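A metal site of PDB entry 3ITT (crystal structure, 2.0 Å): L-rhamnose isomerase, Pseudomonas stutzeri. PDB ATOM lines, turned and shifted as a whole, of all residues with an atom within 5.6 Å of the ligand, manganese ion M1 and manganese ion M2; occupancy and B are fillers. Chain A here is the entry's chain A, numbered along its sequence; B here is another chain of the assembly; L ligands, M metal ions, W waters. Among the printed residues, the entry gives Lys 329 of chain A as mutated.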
ATOM      1  N   TRP A  57      33.614  -2.815 -17.815  1.00  0.00           N
ATOM      2  CA  TRP A  57      32.545  -2.054 -17.187  1.00  0.00           C
ATOM      3  C   TRP A  57      31.181  -2.734 -17.166  1.00  0.00           C
ATOM      4  O   TRP A  57      30.220  -2.213 -16.598  1.00  0.00           O
ATOM      5  CB  TRP A  57      32.425  -0.677 -17.875  1.00  0.00           C
ATOM      6  CG  TRP A  57      32.013  -0.750 -19.311  1.00  0.00           C
ATOM      7  CD1 TRP A  57      30.740  -0.756 -19.805  1.00  0.00           C
ATOM      8  CD2 TRP A  57      32.882  -0.822 -20.457  1.00  0.00           C
ATOM      9  NE1 TRP A  57      30.755  -0.835 -21.183  1.00  0.00           N
ATOM     10  CE2 TRP A  57      32.055  -0.870 -21.604  1.00  0.00           C
ATOM     11  CE3 TRP A  57      34.279  -0.844 -20.615  1.00  0.00           C
ATOM     12  CZ2 TRP A  57      32.583  -0.946 -22.902  1.00  0.00           C
ATOM     13  CZ3 TRP A  57      34.799  -0.925 -21.912  1.00  0.00           C
ATOM     14  CH2 TRP A  57      33.951  -0.972 -23.040  1.00  0.00           C
ATOM     15  N   HIS A 101      38.752   0.191 -19.948  1.00  0.00           N
ATOM     16  CA  HIS A 101      38.331   1.577 -20.063  1.00  0.00           C
ATOM     17  C   HIS A 101      39.197   2.426 -19.141  1.00  0.00           C
ATOM     18  O   HIS A 101      39.338   2.123 -17.967  1.00  0.00           O
ATOM     19  CB  HIS A 101      36.855   1.732 -19.647  1.00  0.00           C
ATOM     20  CG  HIS A 101      36.093   2.707 -20.489  1.00  0.00           C
ATOM     21  ND1 HIS A 101      36.425   4.042 -20.555  1.00  0.00           N
ATOM     22  CD2 HIS A 101      35.045   2.528 -21.332  1.00  0.00           C
ATOM     23  CE1 HIS A 101      35.604   4.648 -21.407  1.00  0.00           C
ATOM     24  NE2 HIS A 101      34.767   3.754 -21.887  1.00  0.00           N
ATOM     25  N   TRP A 104      38.883   4.335 -15.556  1.00  0.00           N
ATOM     26  CA  TRP A 104      38.266   3.405 -14.599  1.00  0.00           C
ATOM     27  C   TRP A 104      39.166   2.224 -14.265  1.00  0.00           C
ATOM     28  O   TRP A 104      39.273   1.811 -13.107  1.00  0.00           O
ATOM     29  CB  TRP A 104      36.942   2.835 -15.123  1.00  0.00           C
ATOM     30  CG  TRP A 104      35.863   3.824 -15.411  1.00  0.00           C
ATOM     31  CD1 TRP A 104      35.689   5.048 -14.844  1.00  0.00           C
ATOM     32  CD2 TRP A 104      34.782   3.650 -16.341  1.00  0.00           C
ATOM     33  NE1 TRP A 104      34.570   5.657 -15.361  1.00  0.00           N
ATOM     34  CE2 TRP A 104      33.993   4.816 -16.281  1.00  0.00           C
ATOM     35  CE3 TRP A 104      34.406   2.624 -17.218  1.00  0.00           C
ATOM     36  CZ2 TRP A 104      32.849   4.989 -17.064  1.00  0.00           C
ATOM     37  CZ3 TRP A 104      33.266   2.789 -17.996  1.00  0.00           C
ATOM     38  CH2 TRP A 104      32.495   3.971 -17.906  1.00  0.00           C
ATOM     39  N   ASN A 127      39.733   1.599 -24.434  1.00  0.00           N
ATOM     40  CA  ASN A 127      38.641   2.553 -24.556  1.00  0.00           C
ATOM     41  C   ASN A 127      39.008   3.836 -23.807  1.00  0.00           C
ATOM     42  O   ASN A 127      39.394   3.801 -22.639  1.00  0.00           O
ATOM     43  CB  ASN A 127      37.351   1.966 -23.962  1.00  0.00           C
ATOM     44  CG  ASN A 127      36.758   0.877 -24.844  1.00  0.00           C
ATOM     45  OD1 ASN A 127      35.999   1.153 -25.773  1.00  0.00           O
ATOM     46  ND2 ASN A 127      37.114  -0.373 -24.561  1.00  0.00           N
ATOM     47  N   SER A 128      38.901   4.968 -24.499  1.00  0.00           N
ATOM     48  CA  SER A 128      39.209   6.254 -23.877  1.00  0.00           C
ATOM     49  C   SER A 128      37.959   6.826 -23.217  1.00  0.00           C
ATOM     50  O   SER A 128      36.829   6.439 -23.549  1.00  0.00           O
ATOM     51  CB  SER A 128      39.747   7.236 -24.911  1.00  0.00           C
ATOM     52  OG  SER A 128      38.814   7.410 -25.966  1.00  0.00           O
ATOM     53  N   PHE A 131      34.114  11.661 -21.801  1.00  0.00           N
ATOM     54  CA  PHE A 131      32.683  11.975 -21.714  1.00  0.00           C
ATOM     55  C   PHE A 131      32.329  12.245 -20.247  1.00  0.00           C
ATOM     56  O   PHE A 131      31.157  12.414 -19.896  1.00  0.00           O
ATOM     57  CB  PHE A 131      31.835  10.823 -22.299  1.00  0.00           C
ATOM     58  CG  PHE A 131      32.149   9.464 -21.735  1.00  0.00           C
ATOM     59  CD1 PHE A 131      31.702   9.091 -20.470  1.00  0.00           C
ATOM     60  CD2 PHE A 131      32.883   8.543 -22.477  1.00  0.00           C
ATOM     61  CE1 PHE A 131      31.975   7.825 -19.952  1.00  0.00           C
ATOM     62  CE2 PHE A 131      33.168   7.273 -21.977  1.00  0.00           C
ATOM     63  CZ  PHE A 131      32.715   6.912 -20.708  1.00  0.00           C
ATOM     64  N   TRP A 179      34.788   6.803 -28.306  1.00  0.00           N
ATOM     65  CA  TRP A 179      33.386   7.204 -28.294  1.00  0.00           C
ATOM     66  C   TRP A 179      33.334   8.408 -27.372  1.00  0.00           C
ATOM     67  O   TRP A 179      33.777   8.326 -26.226  1.00  0.00           O
ATOM     68  CB  TRP A 179      32.447   6.127 -27.730  1.00  0.00           C
ATOM     69  CG  TRP A 179      31.067   6.688 -27.547  1.00  0.00           C
ATOM     70  CD1 TRP A 179      30.162   7.017 -28.530  1.00  0.00           C
ATOM     71  CD2 TRP A 179      30.492   7.171 -26.314  1.00  0.00           C
ATOM     72  NE1 TRP A 179      29.088   7.664 -27.993  1.00  0.00           N
ATOM     73  CE2 TRP A 179      29.258   7.775 -26.631  1.00  0.00           C
ATOM     74  CE3 TRP A 179      30.908   7.130 -24.976  1.00  0.00           C
ATOM     75  CZ2 TRP A 179      28.430   8.349 -25.665  1.00  0.00           C
ATOM     76  CZ3 TRP A 179      30.080   7.705 -24.010  1.00  0.00           C
ATOM     77  CH2 TRP A 179      28.851   8.314 -24.365  1.00  0.00           C
ATOM     78  N   GLU A 219      33.356   5.462 -32.834  1.00  0.00           N
ATOM     79  CA  GLU A 219      32.017   4.922 -32.619  1.00  0.00           C
ATOM     80  C   GLU A 219      30.934   5.993 -32.733  1.00  0.00           C
ATOM     81  O   GLU A 219      30.939   6.970 -31.990  1.00  0.00           O
ATOM     82  CB  GLU A 219      31.940   4.247 -31.251  1.00  0.00           C
ATOM     83  CG  GLU A 219      30.549   3.799 -30.842  1.00  0.00           C
ATOM     84  CD  GLU A 219      30.537   2.977 -29.579  1.00  0.00           C
ATOM     85  OE1 GLU A 219      31.510   3.048 -28.796  1.00  0.00           O
ATOM     86  OE2 GLU A 219      29.541   2.257 -29.354  1.00  0.00           O
ATOM     87  N   LYS A 221      26.985   7.579 -32.635  1.00  0.00           N
ATOM     88  CA  LYS A 221      25.809   7.472 -31.783  1.00  0.00           C
ATOM     89  C   LYS A 221      24.869   8.642 -32.119  1.00  0.00           C
ATOM     90  O   LYS A 221      25.278   9.793 -32.130  1.00  0.00           O
ATOM     91  CB  LYS A 221      26.210   7.505 -30.316  1.00  0.00           C
ATOM     92  CG  LYS A 221      25.125   6.975 -29.382  1.00  0.00           C
ATOM     93  CD  LYS A 221      25.591   7.012 -27.927  1.00  0.00           C
ATOM     94  CE  LYS A 221      24.448   6.639 -26.985  1.00  0.00           C
ATOM     95  NZ  LYS A 221      24.873   6.683 -25.564  1.00  0.00           N
ATOM     96  N   GLU A 224      22.394  11.110 -26.908  1.00  0.00           N
ATOM     97  CA  GLU A 224      22.732  10.748 -25.528  1.00  0.00           C
ATOM     98  C   GLU A 224      24.242  10.556 -25.414  1.00  0.00           C
ATOM     99  O   GLU A 224      24.809   9.636 -26.003  1.00  0.00           O
ATOM    100  CB  GLU A 224      22.029   9.461 -25.051  1.00  0.00           C
ATOM    101  CG  GLU A 224      22.349   9.150 -23.575  1.00  0.00           C
ATOM    102  CD  GLU A 224      22.106   7.705 -23.160  1.00  0.00           C
ATOM    103  OE1 GLU A 224      22.375   6.796 -23.980  1.00  0.00           O
ATOM    104  OE2 GLU A 224      21.680   7.469 -22.010  1.00  0.00           O
ATOM    105  N   LEU A 252      33.191   1.695 -35.861  1.00  0.00           N
ATOM    106  CA  LEU A 252      32.642   0.685 -34.986  1.00  0.00           C
ATOM    107  C   LEU A 252      31.125   0.895 -34.962  1.00  0.00           C
ATOM    108  O   LEU A 252      30.658   2.021 -34.821  1.00  0.00           O
ATOM    109  CB  LEU A 252      33.227   0.831 -33.591  1.00  0.00           C
ATOM    110  CG  LEU A 252      32.823  -0.240 -32.590  1.00  0.00           C
ATOM    111  CD1 LEU A 252      34.067  -0.879 -31.987  1.00  0.00           C
ATOM    112  CD2 LEU A 252      31.934   0.385 -31.512  1.00  0.00           C
ATOM    113  N   ASP A 254      27.659   0.115 -33.079  1.00  0.00           N
ATOM    114  CA  ASP A 254      27.027  -0.340 -31.838  1.00  0.00           C
ATOM    115  C   ASP A 254      25.548  -0.446 -32.178  1.00  0.00           C
ATOM    116  O   ASP A 254      24.909   0.557 -32.508  1.00  0.00           O
ATOM    117  CB  ASP A 254      27.242   0.669 -30.719  1.00  0.00           C
ATOM    118  CG  ASP A 254      26.680   0.179 -29.389  1.00  0.00           C
ATOM    119  OD1 ASP A 254      25.499  -0.237 -29.348  1.00  0.00           O
ATOM    120  OD2 ASP A 254      27.416   0.203 -28.383  1.00  0.00           O
ATOM    121  N   HIS A 257      22.761   2.250 -31.266  1.00  0.00           N
ATOM    122  CA  HIS A 257      23.043   3.666 -31.533  1.00  0.00           C
ATOM    123  C   HIS A 257      22.424   4.246 -32.793  1.00  0.00           C
ATOM    124  O   HIS A 257      22.921   5.247 -33.305  1.00  0.00           O
ATOM    125  CB  HIS A 257      24.569   3.892 -31.605  1.00  0.00           C
ATOM    126  CG  HIS A 257      25.275   3.677 -30.305  1.00  0.00           C
ATOM    127  ND1 HIS A 257      26.602   4.004 -30.122  1.00  0.00           N
ATOM    128  CD2 HIS A 257      24.836   3.209 -29.114  1.00  0.00           C
ATOM    129  CE1 HIS A 257      26.952   3.747 -28.877  1.00  0.00           C
ATOM    130  NE2 HIS A 257      25.892   3.267 -28.241  1.00  0.00           N
ATOM    131  N   HIS A 281      29.707  -3.547 -31.511  1.00  0.00           N
ATOM    132  CA  HIS A 281      29.389  -3.401 -30.108  1.00  0.00           C
ATOM    133  C   HIS A 281      28.026  -4.072 -30.033  1.00  0.00           C
ATOM    134  O   HIS A 281      27.012  -3.495 -30.446  1.00  0.00           O
ATOM    135  CB  HIS A 281      29.281  -1.939 -29.702  1.00  0.00           C
ATOM    136  CG  HIS A 281      30.543  -1.389 -29.111  1.00  0.00           C
ATOM    137  ND1 HIS A 281      30.575  -0.174 -28.455  1.00  0.00           N
ATOM    138  CD2 HIS A 281      31.794  -1.880 -29.068  1.00  0.00           C
ATOM    139  CE1 HIS A 281      31.810   0.047 -28.026  1.00  0.00           C
ATOM    140  NE2 HIS A 281      32.574  -0.972 -28.388  1.00  0.00           N
ATOM    141  N   ASN A 283      24.647  -5.750 -28.436  1.00  0.00           N
ATOM    142  CA  ASN A 283      23.656  -5.504 -27.405  1.00  0.00           C
ATOM    143  C   ASN A 283      22.297  -5.509 -28.087  1.00  0.00           C
ATOM    144  O   ASN A 283      22.221  -5.648 -29.312  1.00  0.00           O
ATOM    145  CB  ASN A 283      23.916  -4.153 -26.701  1.00  0.00           C
ATOM    146  CG  ASN A 283      24.024  -2.984 -27.672  1.00  0.00           C
ATOM    147  OD1 ASN A 283      23.094  -2.697 -28.430  1.00  0.00           O
ATOM    148  ND2 ASN A 283      25.163  -2.298 -27.646  1.00  0.00           N
ATOM    149  N   ASP A 289      19.287   3.579 -26.732  1.00  0.00           N
ATOM    150  CA  ASP A 289      20.530   2.856 -26.487  1.00  0.00           C
ATOM    151  C   ASP A 289      20.326   2.133 -25.163  1.00  0.00           C
ATOM    152  O   ASP A 289      20.996   2.414 -24.169  1.00  0.00           O
ATOM    153  CB  ASP A 289      21.694   3.854 -26.405  1.00  0.00           C
ATOM    154  CG  ASP A 289      23.034   3.173 -26.222  1.00  0.00           C
ATOM    155  OD1 ASP A 289      23.215   2.052 -26.739  1.00  0.00           O
ATOM    156  OD2 ASP A 289      23.911   3.778 -25.569  1.00  0.00           O
ATOM    157  N   ASP A 291      21.090  -0.815 -24.210  1.00  0.00           N
ATOM    158  CA  ASP A 291      22.201  -1.663 -23.773  1.00  0.00           C
ATOM    159  C   ASP A 291      21.776  -2.973 -23.106  1.00  0.00           C
ATOM    160  O   ASP A 291      22.388  -3.414 -22.139  1.00  0.00           O
ATOM    161  CB  ASP A 291      23.104  -0.879 -22.821  1.00  0.00           C
ATOM    162  CG  ASP A 291      23.922   0.164 -23.537  1.00  0.00           C
ATOM    163  OD1 ASP A 291      24.259  -0.087 -24.708  1.00  0.00           O
ATOM    164  OD2 ASP A 291      24.217   1.230 -22.938  1.00  0.00           O
ATOM    165  N   ASP A 327      28.922  -4.589 -25.680  1.00  0.00           N
ATOM    166  CA  ASP A 327      28.830  -3.321 -24.973  1.00  0.00           C
ATOM    167  C   ASP A 327      27.422  -3.242 -24.365  1.00  0.00           C
ATOM    168  O   ASP A 327      26.509  -2.744 -24.993  1.00  0.00           O
ATOM    169  CB  ASP A 327      29.033  -2.136 -25.923  1.00  0.00           C
ATOM    170  CG  ASP A 327      29.132  -0.817 -25.185  1.00  0.00           C
ATOM    171  OD1 ASP A 327      28.897  -0.798 -23.952  1.00  0.00           O
ATOM    172  OD2 ASP A 327      29.433   0.212 -25.828  1.00  0.00           O
ATOM    173  N   LYS A 329      24.967  -3.006 -20.417  1.00  0.00           N
ATOM    174  CA  LYS A 329      24.859  -2.571 -19.039  1.00  0.00           C
ATOM    175  C   LYS A 329      23.759  -3.437 -18.433  1.00  0.00           C
ATOM    176  O   LYS A 329      22.685  -3.581 -19.012  1.00  0.00           O
ATOM    177  CB  LYS A 329      24.466  -1.096 -18.956  1.00  0.00           C
ATOM    178  CG  LYS A 329      25.597  -0.115 -19.203  1.00  0.00           C
ATOM    179  CD  LYS A 329      26.044  -0.059 -20.655  1.00  0.00           C
ATOM    180  CE  LYS A 329      27.020   1.096 -20.863  1.00  0.00           C
ATOM    181  NZ  LYS A 329      27.365   1.286 -22.301  1.00  0.00           N
ATOM    182  N   ARG B  65      23.329   9.357 -17.584  1.00  0.00           N
ATOM    183  CA  ARG B  65      23.912   8.188 -16.946  1.00  0.00           C
ATOM    184  C   ARG B  65      25.427   8.169 -17.165  1.00  0.00           C
ATOM    185  O   ARG B  65      26.135   7.420 -16.498  1.00  0.00           O
ATOM    186  CB  ARG B  65      23.276   6.916 -17.498  1.00  0.00           C
ATOM    187  CG  ARG B  65      23.372   6.767 -18.996  1.00  0.00           C
ATOM    188  CD  ARG B  65      22.785   5.439 -19.452  1.00  0.00           C
ATOM    189  NE  ARG B  65      22.808   5.330 -20.904  1.00  0.00           N
ATOM    190  CZ  ARG B  65      23.101   4.228 -21.572  1.00  0.00           C
ATOM    191  NH1 ARG B  65      23.403   3.105 -20.918  1.00  0.00           N
ATOM    192  NH2 ARG B  65      23.106   4.242 -22.899  1.00  0.00           N
ATOM    193  N   PHE B  66      25.917   9.000 -18.081  1.00  0.00           N
ATOM    194  CA  PHE B  66      27.347   9.064 -18.382  1.00  0.00           C
ATOM    195  C   PHE B  66      28.118  10.083 -17.544  1.00  0.00           C
ATOM    196  O   PHE B  66      29.306   9.887 -17.269  1.00  0.00           O
ATOM    197  CB  PHE B  66      27.561   9.391 -19.860  1.00  0.00           C
ATOM    198  CG  PHE B  66      27.156   8.282 -20.778  1.00  0.00           C
ATOM    199  CD1 PHE B  66      27.953   7.132 -20.903  1.00  0.00           C
ATOM    200  CD2 PHE B  66      25.961   8.346 -21.500  1.00  0.00           C
ATOM    201  CE1 PHE B  66      27.562   6.081 -21.722  1.00  0.00           C
ATOM    202  CE2 PHE B  66      25.568   7.299 -22.311  1.00  0.00           C
ATOM    203  CZ  PHE B  66      26.371   6.163 -22.420  1.00  0.00           C
HETATM  204  C1  LIG L   1      28.005   4.826 -25.265  1.00  0.00           C
HETATM  205  C2  LIG L   1      28.851   3.906 -26.147  1.00  0.00           C
HETATM  206  C3  LIG L   1      30.217   3.669 -25.519  1.00  0.00           C
HETATM  207  C4  LIG L   1      30.131   3.451 -24.006  1.00  0.00           C
HETATM  208  C5  LIG L   1      31.494   2.961 -23.484  1.00  0.00           C
HETATM  209  C6  LIG L   1      31.394   2.724 -21.988  1.00  0.00           C
HETATM  210  O1  LIG L   1      26.789   4.843 -25.382  1.00  0.00           O
HETATM  211  O2  LIG L   1      28.186   2.667 -26.331  1.00  0.00           O
HETATM  212  O3  LIG L   1      30.846   2.559 -26.132  1.00  0.00           O
HETATM  213  O4  LIG L   1      29.126   2.498 -23.705  1.00  0.00           O
HETATM  214  O5  LIG L   1      32.515   3.907 -23.768  1.00  0.00           O
HETATM  215 MN    MN M   1      29.362   0.998 -27.694  1.00  0.00          MN
HETATM  216 MN    MN M   2      25.852   2.960 -26.248  1.00  0.00          MN
HETATM  217  O   HOH W   1      26.132   2.618 -24.040  1.00  0.00           O
HETATM  218  O   HOH W   2      25.708   1.127 -25.951  1.00  0.00           O
HETATM  219  O   HOH W   3      34.024   3.261 -25.708  1.00  0.00           O
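NZ of Lys 221 sits close to O1 of the ligand. The side-chain amino group of Lys 329 is in hydrogen-bond range of an oxygen (O4) of the ligand, 2.6 Å away. A ring nitrogen (NE2) of His 101 lies within hydrogen-bond range of an oxygen (O5) of the ligand, at 2.9 Å.
OD1 of Asp 327 sits at hydrogen-bond distance from NE1 of Trp 57 (3.3 Å). The side-chain amide nitrogen of Asn 283 sits at hydrogen-bond distance from the backbone carbonyl oxygen of Asp 327 (3.0 Å). NZ of Lys 329 is in salt-bridge range of OD1 of Asp 327, at 3.1 Å. The guanidinium group (NH1) of Arg 65 of chain B is in salt-bridge range of the side-chain carboxylate (OD2) of Asp 291 (2.9 Å). OD2 of Asp 289 sits close to NZ of Lys 221. NZ of Lys 329 is in salt-bridge range of OD2 of Asp 291, 3.2 Å away. NH2 of Arg 65 of chain B sits at hydrogen-bond distance from O of Asp 289, 3.1 Å away. The side-chain carboxylate (OD1) of Asp 254 sits at hydrogen-bond distance from the side-chain amide nitrogen (ND2) of Asn 283.
Residues that only touch the ligand: Phe 66 of chain B (3.3 Å), Trp 179 (3.5 Å), Trp 57 (3.7 Å) and Phe 131 (3.9 Å). Hydrophobic or aromatic side chains within 4 Å of the ligand: Trp 57, His 101, Phe 131, Trp 179, His 257, His 281 and Phe 66 of chain B. Of the 21 residues printed, 13 come within 4 Å of the ligand. The nearest printed residue that does not touch the ligand is Trp 104 (4.4 Å).
The nearest printed residue that does not touch manganese ion M1 is Leu 252 (4.6 Å).
Residues that only touch manganese ion M2: Lys 221 and Asp 291. Within 4 Å of manganese ion M2: Lys 221, Asp 254, His 257, Asp 289 and Asp 291. The nearest printed residue that does not touch manganese ion M2 is Arg 65 of chain B (4.5 Å).
Manganese ion M1 is bound by a ring nitrogen (ND1) of His 281, the side-chain carboxylate of Asp 327, the side-chain carboxylate of Glu 219, the side-chain carboxylate of Asp 254, an oxygen (O2) of the ligand and an oxygen (O3) of the ligand. Manganese ion M1 has six donor atoms within binding distance.
Manganese ion M2 is bound by water W2 (1.9 Å), NE2 of His 257 (2.0 Å), OD2 of Asp 289 (2.2 Å), water W1 (2.3 Å), O1 of the ligand (2.3 Å) and O2 of the ligand (2.4 Å). Slightly farther from manganese ion M2 lies the side-chain carboxylate (OD1) of Asp 289 (2.8 Å).
Water W2 bridges the side-chain carboxylate (OD1) of Asp 289 (2.8 Å) and the side-chain carboxylate (OD2) of Asp 291 (3.4 Å). Water W1 lies within hydrogen-bond range of the side-chain amino group of Lys 329 (2.5 Å), the side-chain carboxylate of Asp 291 (2.6 Å) and an oxygen (O4) of the ligand (3.0 Å). Water W3 bridges an oxygen (O5) of the ligand and the side-chain amide oxygen of Asn 127.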
